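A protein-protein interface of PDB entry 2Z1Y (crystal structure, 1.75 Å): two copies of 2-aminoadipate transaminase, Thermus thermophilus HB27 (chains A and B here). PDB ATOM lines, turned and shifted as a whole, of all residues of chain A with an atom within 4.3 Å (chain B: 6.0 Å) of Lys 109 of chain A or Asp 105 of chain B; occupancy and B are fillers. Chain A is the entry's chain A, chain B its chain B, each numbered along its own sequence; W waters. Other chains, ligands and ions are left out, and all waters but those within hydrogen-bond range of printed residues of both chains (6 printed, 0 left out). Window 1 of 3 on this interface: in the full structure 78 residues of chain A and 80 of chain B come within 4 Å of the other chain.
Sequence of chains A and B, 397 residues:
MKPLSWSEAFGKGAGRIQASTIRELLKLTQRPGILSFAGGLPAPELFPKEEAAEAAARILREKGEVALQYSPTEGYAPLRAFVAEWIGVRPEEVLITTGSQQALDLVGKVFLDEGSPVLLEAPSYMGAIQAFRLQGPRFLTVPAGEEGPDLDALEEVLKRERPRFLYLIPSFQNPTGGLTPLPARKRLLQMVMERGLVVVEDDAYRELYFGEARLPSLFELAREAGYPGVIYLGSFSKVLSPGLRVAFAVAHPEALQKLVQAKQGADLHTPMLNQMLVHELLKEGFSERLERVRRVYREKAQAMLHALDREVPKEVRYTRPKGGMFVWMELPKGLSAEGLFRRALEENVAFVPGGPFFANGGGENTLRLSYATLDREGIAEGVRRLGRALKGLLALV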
ATOM      1  N   ASP A 105      -6.538 -13.524 -26.096  1.00  0.00           N
ATOM      2  CA  ASP A 105      -5.333 -14.295 -26.406  1.00  0.00           C
ATOM      3  C   ASP A 105      -5.195 -14.472 -27.921  1.00  0.00           C
ATOM      4  O   ASP A 105      -4.094 -14.292 -28.459  1.00  0.00           O
ATOM      5  CB  ASP A 105      -5.324 -15.664 -25.742  1.00  0.00           C
ATOM      6  CG  ASP A 105      -3.938 -16.359 -25.753  1.00  0.00           C
ATOM      7  OD1 ASP A 105      -2.923 -15.675 -25.657  1.00  0.00           O
ATOM      8  OD2 ASP A 105      -3.923 -17.470 -25.909  1.00  0.00           O
ATOM      9  N   LEU A 106      -6.295 -14.766 -28.614  1.00  0.00           N
ATOM     10  CA  LEU A 106      -6.261 -14.967 -30.078  1.00  0.00           C
ATOM     11  C   LEU A 106      -5.837 -13.679 -30.795  1.00  0.00           C
ATOM     12  O   LEU A 106      -5.026 -13.693 -31.752  1.00  0.00           O
ATOM     13  CB  LEU A 106      -7.543 -15.523 -30.634  1.00  0.00           C
ATOM     14  CG  LEU A 106      -7.985 -16.865 -30.029  1.00  0.00           C
ATOM     15  CD1 LEU A 106      -9.347 -17.232 -30.560  1.00  0.00           C
ATOM     16  CD2 LEU A 106      -7.052 -17.977 -30.293  1.00  0.00           C
ATOM     17  N   VAL A 107      -6.438 -12.549 -30.374  1.00  0.00           N
ATOM     18  CA  VAL A 107      -6.053 -11.245 -30.866  1.00  0.00           C
ATOM     19  C   VAL A 107      -4.599 -10.970 -30.663  1.00  0.00           C
ATOM     20  O   VAL A 107      -3.928 -10.506 -31.601  1.00  0.00           O
ATOM     21  CB  VAL A 107      -6.960 -10.163 -30.229  1.00  0.00           C
ATOM     22  CG1 VAL A 107      -6.361  -8.794 -30.448  1.00  0.00           C
ATOM     23  CG2 VAL A 107      -8.346 -10.270 -30.855  1.00  0.00           C
ATOM     24  N   GLY A 108      -4.064 -11.237 -29.456  1.00  0.00           N
ATOM     25  CA  GLY A 108      -2.637 -11.013 -29.237  1.00  0.00           C
ATOM     26  C   GLY A 108      -1.784 -11.818 -30.212  1.00  0.00           C
ATOM     27  O   GLY A 108      -0.783 -11.338 -30.791  1.00  0.00           O
ATOM     28  N   LYS A 109      -2.163 -13.090 -30.378  1.00  0.00           N
ATOM     29  CA  LYS A 109      -1.428 -13.981 -31.262  1.00  0.00           C
ATOM     30  C   LYS A 109      -1.416 -13.531 -32.727  1.00  0.00           C
ATOM     31  O   LYS A 109      -0.362 -13.682 -33.435  1.00  0.00           O
ATOM     32  CB  LYS A 109      -2.060 -15.381 -31.187  1.00  0.00           C
ATOM     33  CG  LYS A 109      -1.764 -16.144 -29.908  1.00  0.00           C
ATOM     34  CD  LYS A 109      -2.660 -17.385 -29.819  1.00  0.00           C
ATOM     35  CE  LYS A 109      -2.225 -18.282 -28.638  1.00  0.00           C
ATOM     36  NZ  LYS A 109      -3.091 -19.448 -28.490  1.00  0.00           N
ATOM     37  N   VAL A 110      -2.545 -13.023 -33.207  1.00  0.00           N
ATOM     38  CA  VAL A 110      -2.718 -12.678 -34.608  1.00  0.00           C
ATOM     39  C   VAL A 110      -2.037 -11.335 -34.934  1.00  0.00           C
ATOM     40  O   VAL A 110      -1.574 -11.147 -36.066  1.00  0.00           O
ATOM     41  CB  VAL A 110      -4.203 -12.693 -34.959  1.00  0.00           C
ATOM     42  CG1 VAL A 110      -4.470 -12.091 -36.323  1.00  0.00           C
ATOM     43  CG2 VAL A 110      -4.779 -14.111 -34.944  1.00  0.00           C
ATOM     44  N   PHE A 111      -2.056 -10.384 -33.983  1.00  0.00           N
ATOM     45  CA  PHE A 111      -1.670  -9.009 -34.247  1.00  0.00           C
ATOM     46  C   PHE A 111      -0.341  -8.542 -33.680  1.00  0.00           C
ATOM     47  O   PHE A 111       0.129  -7.494 -34.179  1.00  0.00           O
ATOM     48  CB  PHE A 111      -2.753  -7.980 -33.850  1.00  0.00           C
ATOM     49  CG  PHE A 111      -4.001  -8.031 -34.700  1.00  0.00           C
ATOM     50  CD1 PHE A 111      -4.129  -7.339 -35.881  1.00  0.00           C
ATOM     51  CD2 PHE A 111      -5.051  -8.843 -34.320  1.00  0.00           C
ATOM     52  CE1 PHE A 111      -5.283  -7.401 -36.642  1.00  0.00           C
ATOM     53  CE2 PHE A 111      -6.204  -8.876 -35.060  1.00  0.00           C
ATOM     54  CZ  PHE A 111      -6.298  -8.218 -36.270  1.00  0.00           C
ATOM     55  N   GLN A 135       3.114 -11.554 -25.830  1.00  0.00           N
ATOM     56  CA  GLN A 135       3.698 -11.382 -27.132  1.00  0.00           C
ATOM     57  C   GLN A 135       4.885 -10.410 -27.063  1.00  0.00           C
ATOM     58  O   GLN A 135       5.560 -10.158 -28.075  1.00  0.00           O
ATOM     59  CB  GLN A 135       2.646 -10.879 -28.136  1.00  0.00           C
ATOM     60  CG  GLN A 135       1.355 -11.717 -28.185  1.00  0.00           C
ATOM     61  CD  GLN A 135       1.610 -13.169 -28.566  1.00  0.00           C
ATOM     62  OE1 GLN A 135       0.854 -14.122 -28.206  1.00  0.00           O
ATOM     63  NE2 GLN A 135       2.727 -13.376 -29.234  1.00  0.00           N
ATOM     64  N   GLY A 265      -5.316 -24.392 -32.809  1.00  0.00           N
ATOM     65  CA  GLY A 265      -4.225 -24.928 -32.007  1.00  0.00           C
ATOM     66  C   GLY A 265      -4.311 -24.483 -30.539  1.00  0.00           C
ATOM     67  O   GLY A 265      -3.508 -24.928 -29.739  1.00  0.00           O
ATOM     68  N   ALA A 266      -5.264 -23.595 -30.203  1.00  0.00           N
ATOM     69  CA  ALA A 266      -5.438 -23.138 -28.846  1.00  0.00           C
ATOM     70  C   ALA A 266      -6.224 -24.201 -28.045  1.00  0.00           C
ATOM     71  O   ALA A 266      -5.844 -24.550 -26.888  1.00  0.00           O
ATOM     72  CB  ALA A 266      -6.162 -21.769 -28.843  1.00  0.00           C
ATOM     73  N   GLY B  11       0.390  -9.480 -37.350  1.00  0.00           N
ATOM     74  CA  GLY B  11       1.747  -9.727 -36.954  1.00  0.00           C
ATOM     75  C   GLY B  11       2.273 -11.058 -37.497  1.00  0.00           C
ATOM     76  O   GLY B  11       1.611 -11.685 -38.272  1.00  0.00           O
ATOM     77  N   LYS B  12       3.435 -11.520 -37.032  1.00  0.00           N
ATOM     78  CA  LYS B  12       4.065 -12.700 -37.585  1.00  0.00           C
ATOM     79  C   LYS B  12       3.215 -13.944 -37.305  1.00  0.00           C
ATOM     80  O   LYS B  12       3.253 -14.920 -38.060  1.00  0.00           O
ATOM     81  CB  LYS B  12       5.466 -12.867 -37.046  1.00  0.00           C
ATOM     82  CG  LYS B  12       6.417 -11.783 -37.577  1.00  0.00           C
ATOM     83  CD  LYS B  12       7.828 -11.871 -37.043  1.00  0.00           C
ATOM     84  CE  LYS B  12       7.923 -11.484 -35.587  1.00  0.00           C
ATOM     85  NZ  LYS B  12       9.224 -10.928 -35.201  1.00  0.00           N
ATOM     86  N   GLY B  13       2.490 -13.917 -36.199  1.00  0.00           N
ATOM     87  CA  GLY B  13       1.730 -15.106 -35.823  1.00  0.00           C
ATOM     88  C   GLY B  13       0.689 -15.475 -36.866  1.00  0.00           C
ATOM     89  O   GLY B  13       0.381 -16.676 -37.023  1.00  0.00           O
ATOM     90  N   ALA B  14       0.105 -14.468 -37.552  1.00  0.00           N
ATOM     91  CA  ALA B  14      -0.905 -14.680 -38.583  1.00  0.00           C
ATOM     92  C   ALA B  14      -0.369 -15.493 -39.755  1.00  0.00           C
ATOM     93  O   ALA B  14      -1.143 -16.191 -40.385  1.00  0.00           O
ATOM     94  CB  ALA B  14      -1.443 -13.311 -39.055  1.00  0.00           C
ATOM     95  N   SER B 100      -5.961 -31.522 -24.108  1.00  0.00           N
ATOM     96  CA  SER B 100      -4.517 -31.545 -24.131  1.00  0.00           C
ATOM     97  C   SER B 100      -4.007 -30.643 -25.267  1.00  0.00           C
ATOM     98  O   SER B 100      -2.860 -30.205 -25.198  1.00  0.00           O
ATOM     99  CB  SER B 100      -3.964 -32.988 -24.083  1.00  0.00           C
ATOM    100  OG  SER B 100      -4.514 -33.678 -25.191  1.00  0.00           O
ATOM    101  N   GLN B 101      -4.843 -30.301 -26.247  1.00  0.00           N
ATOM    102  CA  GLN B 101      -4.429 -29.348 -27.250  1.00  0.00           C
ATOM    103  C   GLN B 101      -4.022 -28.048 -26.552  1.00  0.00           C
ATOM    104  O   GLN B 101      -3.070 -27.388 -26.927  1.00  0.00           O
ATOM    105  CB  GLN B 101      -5.520 -29.087 -28.280  1.00  0.00           C
ATOM    106  CG  GLN B 101      -5.090 -28.154 -29.410  1.00  0.00           C
ATOM    107  CD  GLN B 101      -3.867 -28.572 -30.166  1.00  0.00           C
ATOM    108  OE1 GLN B 101      -2.936 -27.787 -30.516  1.00  0.00           O
ATOM    109  NE2 GLN B 101      -3.882 -29.810 -30.484  1.00  0.00           N
ATOM    110  N   GLN B 102      -4.781 -27.665 -25.520  1.00  0.00           N
ATOM    111  CA  GLN B 102      -4.368 -26.461 -24.810  1.00  0.00           C
ATOM    112  C   GLN B 102      -3.049 -26.615 -24.091  1.00  0.00           C
ATOM    113  O   GLN B 102      -2.223 -25.712 -24.117  1.00  0.00           O
ATOM    114  CB  GLN B 102      -5.455 -26.068 -23.834  1.00  0.00           C
ATOM    115  CG  GLN B 102      -5.011 -24.923 -22.919  1.00  0.00           C
ATOM    116  CD  GLN B 102      -6.097 -24.394 -22.004  1.00  0.00           C
ATOM    117  OE1 GLN B 102      -6.366 -24.994 -20.951  1.00  0.00           O
ATOM    118  NE2 GLN B 102      -6.664 -23.270 -22.432  1.00  0.00           N
ATOM    119  N   ALA B 103      -2.817 -27.756 -23.479  1.00  0.00           N
ATOM    120  CA  ALA B 103      -1.546 -28.071 -22.847  1.00  0.00           C
ATOM    121  C   ALA B 103      -0.419 -27.863 -23.839  1.00  0.00           C
ATOM    122  O   ALA B 103       0.621 -27.284 -23.510  1.00  0.00           O
ATOM    123  CB  ALA B 103      -1.526 -29.466 -22.206  1.00  0.00           C
ATOM    124  N   LEU B 104      -0.654 -28.294 -25.081  1.00  0.00           N
ATOM    125  CA  LEU B 104       0.367 -28.129 -26.109  1.00  0.00           C
ATOM    126  C   LEU B 104       0.661 -26.678 -26.356  1.00  0.00           C
ATOM    127  O   LEU B 104       1.825 -26.255 -26.463  1.00  0.00           O
ATOM    128  CB  LEU B 104      -0.036 -28.904 -27.381  1.00  0.00           C
ATOM    129  CG  LEU B 104      -0.049 -30.433 -27.240  1.00  0.00           C
ATOM    130  CD1 LEU B 104      -0.729 -31.050 -28.453  1.00  0.00           C
ATOM    131  CD2 LEU B 104       1.349 -31.048 -27.017  1.00  0.00           C
ATOM    132  N   ASP B 105      -0.408 -25.865 -26.523  1.00  0.00           N
ATOM    133  CA  ASP B 105      -0.272 -24.439 -26.744  1.00  0.00           C
ATOM    134  C   ASP B 105       0.431 -23.802 -25.534  1.00  0.00           C
ATOM    135  O   ASP B 105       1.344 -23.002 -25.728  1.00  0.00           O
ATOM    136  CB  ASP B 105      -1.627 -23.804 -26.970  1.00  0.00           C
ATOM    137  CG  ASP B 105      -1.557 -22.344 -27.448  1.00  0.00           C
ATOM    138  OD1 ASP B 105      -0.616 -22.024 -28.251  1.00  0.00           O
ATOM    139  OD2 ASP B 105      -2.255 -21.664 -26.885  1.00  0.00           O
ATOM    140  N   LEU B 106       0.128 -24.252 -24.313  1.00  0.00           N
ATOM    141  CA  LEU B 106       0.794 -23.698 -23.104  1.00  0.00           C
ATOM    142  C   LEU B 106       2.286 -23.996 -23.056  1.00  0.00           C
ATOM    143  O   LEU B 106       3.127 -23.101 -22.796  1.00  0.00           O
ATOM    144  CB  LEU B 106       0.118 -24.163 -21.803  1.00  0.00           C
ATOM    145  CG  LEU B 106      -1.362 -23.735 -21.697  1.00  0.00           C
ATOM    146  CD1 LEU B 106      -1.868 -24.295 -20.408  1.00  0.00           C
ATOM    147  CD2 LEU B 106      -1.602 -22.255 -21.795  1.00  0.00           C
ATOM    148  N   VAL B 107       2.623 -25.228 -23.460  1.00  0.00           N
ATOM    149  CA  VAL B 107       4.009 -25.657 -23.526  1.00  0.00           C
ATOM    150  C   VAL B 107       4.693 -24.793 -24.574  1.00  0.00           C
ATOM    151  O   VAL B 107       5.844 -24.386 -24.363  1.00  0.00           O
ATOM    152  CB  VAL B 107       4.096 -27.165 -23.868  1.00  0.00           C
ATOM    153  CG1 VAL B 107       5.485 -27.563 -24.366  1.00  0.00           C
ATOM    154  CG2 VAL B 107       3.694 -28.003 -22.689  1.00  0.00           C
ATOM    155  N   GLY B 108       4.076 -24.564 -25.743  1.00  0.00           N
ATOM    156  CA  GLY B 108       4.750 -23.768 -26.741  1.00  0.00           C
ATOM    157  C   GLY B 108       5.071 -22.365 -26.224  1.00  0.00           C
ATOM    158  O   GLY B 108       6.172 -21.813 -26.470  1.00  0.00           O
ATOM    159  N   LYS B 109       4.051 -21.766 -25.582  1.00  0.00           N
ATOM    160  CA  LYS B 109       4.194 -20.443 -24.986  1.00  0.00           C
ATOM    161  C   LYS B 109       5.345 -20.312 -23.987  1.00  0.00           C
ATOM    162  O   LYS B 109       6.032 -19.275 -23.968  1.00  0.00           O
ATOM    163  CB  LYS B 109       2.872 -20.041 -24.331  1.00  0.00           C
ATOM    164  CG  LYS B 109       1.803 -19.768 -25.351  1.00  0.00           C
ATOM    165  CD  LYS B 109       0.452 -19.600 -24.654  1.00  0.00           C
ATOM    166  CE  LYS B 109      -0.704 -19.122 -25.527  1.00  0.00           C
ATOM    167  NZ  LYS B 109      -1.979 -18.995 -24.824  1.00  0.00           N
ATOM    168  N   VAL B 110       5.505 -21.356 -23.175  1.00  0.00           N
ATOM    169  CA  VAL B 110       6.420 -21.276 -22.053  1.00  0.00           C
ATOM    170  C   VAL B 110       7.860 -21.566 -22.476  1.00  0.00           C
ATOM    171  O   VAL B 110       8.801 -21.057 -21.892  1.00  0.00           O
ATOM    172  CB  VAL B 110       5.954 -22.247 -20.968  1.00  0.00           C
ATOM    173  CG1 VAL B 110       7.039 -22.560 -19.962  1.00  0.00           C
ATOM    174  CG2 VAL B 110       4.722 -21.704 -20.241  1.00  0.00           C
ATOM    175  N   ALA B 131       0.470 -25.987 -32.729  1.00  0.00           N
ATOM    176  CA  ALA B 131       0.692 -25.219 -31.537  1.00  0.00           C
ATOM    177  C   ALA B 131       2.109 -24.646 -31.490  1.00  0.00           C
ATOM    178  O   ALA B 131       2.282 -23.493 -31.165  1.00  0.00           O
ATOM    179  CB  ALA B 131       0.496 -26.101 -30.332  1.00  0.00           C
ATOM    180  N   PHE B 132       3.126 -25.489 -31.745  1.00  0.00           N
ATOM    181  CA  PHE B 132       4.488 -25.050 -31.618  1.00  0.00           C
ATOM    182  C   PHE B 132       4.866 -24.066 -32.715  1.00  0.00           C
ATOM    183  O   PHE B 132       5.703 -23.166 -32.466  1.00  0.00           O
ATOM    184  CB  PHE B 132       5.426 -26.274 -31.641  1.00  0.00           C
ATOM    185  CG  PHE B 132       5.143 -27.317 -30.558  1.00  0.00           C
ATOM    186  CD1 PHE B 132       4.430 -26.989 -29.395  1.00  0.00           C
ATOM    187  CD2 PHE B 132       5.650 -28.603 -30.665  1.00  0.00           C
ATOM    188  CE1 PHE B 132       4.138 -27.968 -28.433  1.00  0.00           C
ATOM    189  CE2 PHE B 132       5.362 -29.564 -29.683  1.00  0.00           C
ATOM    190  CZ  PHE B 132       4.631 -29.242 -28.562  1.00  0.00           C
ATOM    191  N   LEU B 134       3.330 -21.739 -33.992  1.00  0.00           N
ATOM    192  CA  LEU B 134       2.923 -20.397 -33.631  1.00  0.00           C
ATOM    193  C   LEU B 134       4.093 -19.567 -33.090  1.00  0.00           C
ATOM    194  O   LEU B 134       4.101 -18.370 -33.252  1.00  0.00           O
ATOM    195  CB  LEU B 134       1.797 -20.459 -32.607  1.00  0.00           C
ATOM    196  CG  LEU B 134       1.352 -19.096 -32.056  1.00  0.00           C
ATOM    197  CD1 LEU B 134       0.839 -18.154 -33.170  1.00  0.00           C
ATOM    198  CD2 LEU B 134       0.273 -19.247 -31.004  1.00  0.00           C
ATOM    199  N   GLN B 135       5.050 -20.174 -32.413  1.00  0.00           N
ATOM    200  CA  GLN B 135       6.136 -19.478 -31.763  1.00  0.00           C
ATOM    201  C   GLN B 135       7.321 -19.264 -32.713  1.00  0.00           C
ATOM    202  O   GLN B 135       8.337 -18.689 -32.281  1.00  0.00           O
ATOM    203  CB  GLN B 135       6.608 -20.219 -30.519  1.00  0.00           C
ATOM    204  CG  GLN B 135       5.480 -20.626 -29.559  1.00  0.00           C
ATOM    205  CD  GLN B 135       4.667 -19.473 -29.037  1.00  0.00           C
ATOM    206  OE1 GLN B 135       3.471 -19.553 -28.658  1.00  0.00           O
ATOM    207  NE2 GLN B 135       5.297 -18.334 -29.057  1.00  0.00           N
ATOM    208  N   ALA B 266      -4.983 -17.551 -21.184  1.00  0.00           N
ATOM    209  CA  ALA B 266      -5.474 -18.336 -22.300  1.00  0.00           C
ATOM    210  C   ALA B 266      -7.000 -18.401 -22.262  1.00  0.00           C
ATOM    211  O   ALA B 266      -7.646 -18.215 -23.298  1.00  0.00           O
ATOM    212  CB  ALA B 266      -4.871 -19.706 -22.281  1.00  0.00           C
HETATM  213  O   HOH W   1       1.392 -11.944 -34.545  1.00  0.00           O
HETATM  214  O   HOH W   2       3.280 -16.312 -31.041  1.00  0.00           O
HETATM  215  O   HOH W   3      -5.651 -22.232 -24.976  1.00  0.00           O
HETATM  216  O   HOH W   4       5.560 -15.257 -29.517  1.00  0.00           O
HETATM  217  O   HOH W   5      -1.414 -22.772 -30.619  1.00  0.00           O
HETATM  218  O   HOH W   6       1.965 -16.948 -28.435  1.00  0.00           O
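The side-chain carboxylate of Asp 105 of chain A lies within salt-bridge range of the side-chain amino group of Lys 109 of chain B (2.7 Å).
The side-chain amino group (NZ) of Lys 109 of chain A lies within salt-bridge range of the side-chain carboxylate (OD2) of Asp 105 of chain B, at 2.9 Å.
The backbone carbonyl oxygen (O) of Val 110 of chain A is in hydrogen-bond range of the backbone NH (N) of Gly 11 of chain B, 2.9 Å away.
The backbone carbonyl oxygen of Gly 265 of chain A sits close to the side-chain amide oxygen of Gln 101 of chain B, 3.0 Å away.
Water W5 lies within hydrogen-bond range of OD1 of Asp 105 of chain B (2.6 Å) and O of Gly 265 of chain A (3.1 Å).
Water W1 lies within hydrogen-bond range of O of Lys 109 of chain A (2.7 Å), N of Gly 13 of chain B (2.8 Å), N of Lys 12 of chain B (3.2 Å) and O of Val 110 of chain A (3.4 Å).
Water W3 bridges the side-chain amide nitrogen (NE2) of Gln 102 of chain B and the backbone carbonyl oxygen (O) of Ala 266 of chain A.
Water W6 bridges OE1 of Gln 135 of chain B (3.0 Å) and OE1 of Gln 135 of chain A (3.0 Å).
Water W4 lies within hydrogen-bond range of the side-chain amide nitrogen (NE2) of Gln 135 of chain B (3.1 Å) and the side-chain amide nitrogen (NE2) of Gln 135 of chain A (3.4 Å).
Water W2 lies within hydrogen-bond range of the backbone carbonyl oxygen (O) of Leu 134 of chain B (3.1 Å), the side-chain amide nitrogen (NE2) of Gln 135 of chain B (3.5 Å) and the side-chain amide nitrogen (NE2) of Gln 135 of chain A (3.5 Å).
The side-chain carboxylate of Asp 105 of chain A is in salt-bridge range of the side-chain amino group of Lys 109 of chain A (3.4 Å).
The side-chain carboxylate (OD2) of Asp 105 of chain B is in salt-bridge range of the side-chain amino group (NZ) of Lys 109 of chain B.
Among the printed residues, merely in contact across the chains: Lys 109 of chain A with Gly 13 of chain B (3.5 Å), Lys 109 of chain A with Lys 109 of chain B (3.6 Å), Lys 109 of chain A with Leu 134 of chain B (3.6 Å), Val 110 of chain A with Ala 14 of chain B (3.7 Å), Phe 111 of chain A with Gly 11 of chain B (3.8 Å), Gly 265 of chain A with Asp 105 of chain B (3.5 Å), Ala 266 of chain A with Gln 101 of chain B (3.96 Å) and Ala 266 of chain A with Gln 102 of chain B (3.2 Å).
Of the 10 printed residues of chain A, 6 touch a printed residue of chain B.
Printed residues of chain B that touch a printed residue of chain A: Gly 11, Gly 13, Ala 14, Gln 101, Gln 102, Asp 105, Lys 109 and Leu 134.
Hydrophobic or aromatic side chains of chain B that line the printed part of chain A: Ala 14 and Leu 134.
Among the printed residues, 12 pairs touch across the chains.
Asp 105 of chain A touches Lys 109 of chain B, and with the chains exchanged Lys 109 of chain A touches Asp 105 of chain B.
Lys 109 of chain B touches its own counterpart, Lys 109 of chain A.
Positions printed for both chains: 105, 106, 107, 108, 109, 110, 135 and 266.
Printed residues of chain B within 4 Å of Asp 105 of chain A: Lys 109 (2.7 Å).
Of the printed residues of chain B, Gly 265 of chain A touches Gln 101 and Asp 105.
Of the printed residues of chain A, Gly 13 of chain B touches Lys 109.
Of the printed residues of chain A, Gln 101 of chain B touches Gly 265 (3.0 Å) and Ala 266 (3.96 Å).
Printed residues of chain A within 4 Å of Asp 105 of chain B: Lys 109 (2.9 Å) and Gly 265 (3.5 Å).
Of the printed residues of chain A, Lys 109 of chain B touches Asp 105 and Lys 109.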
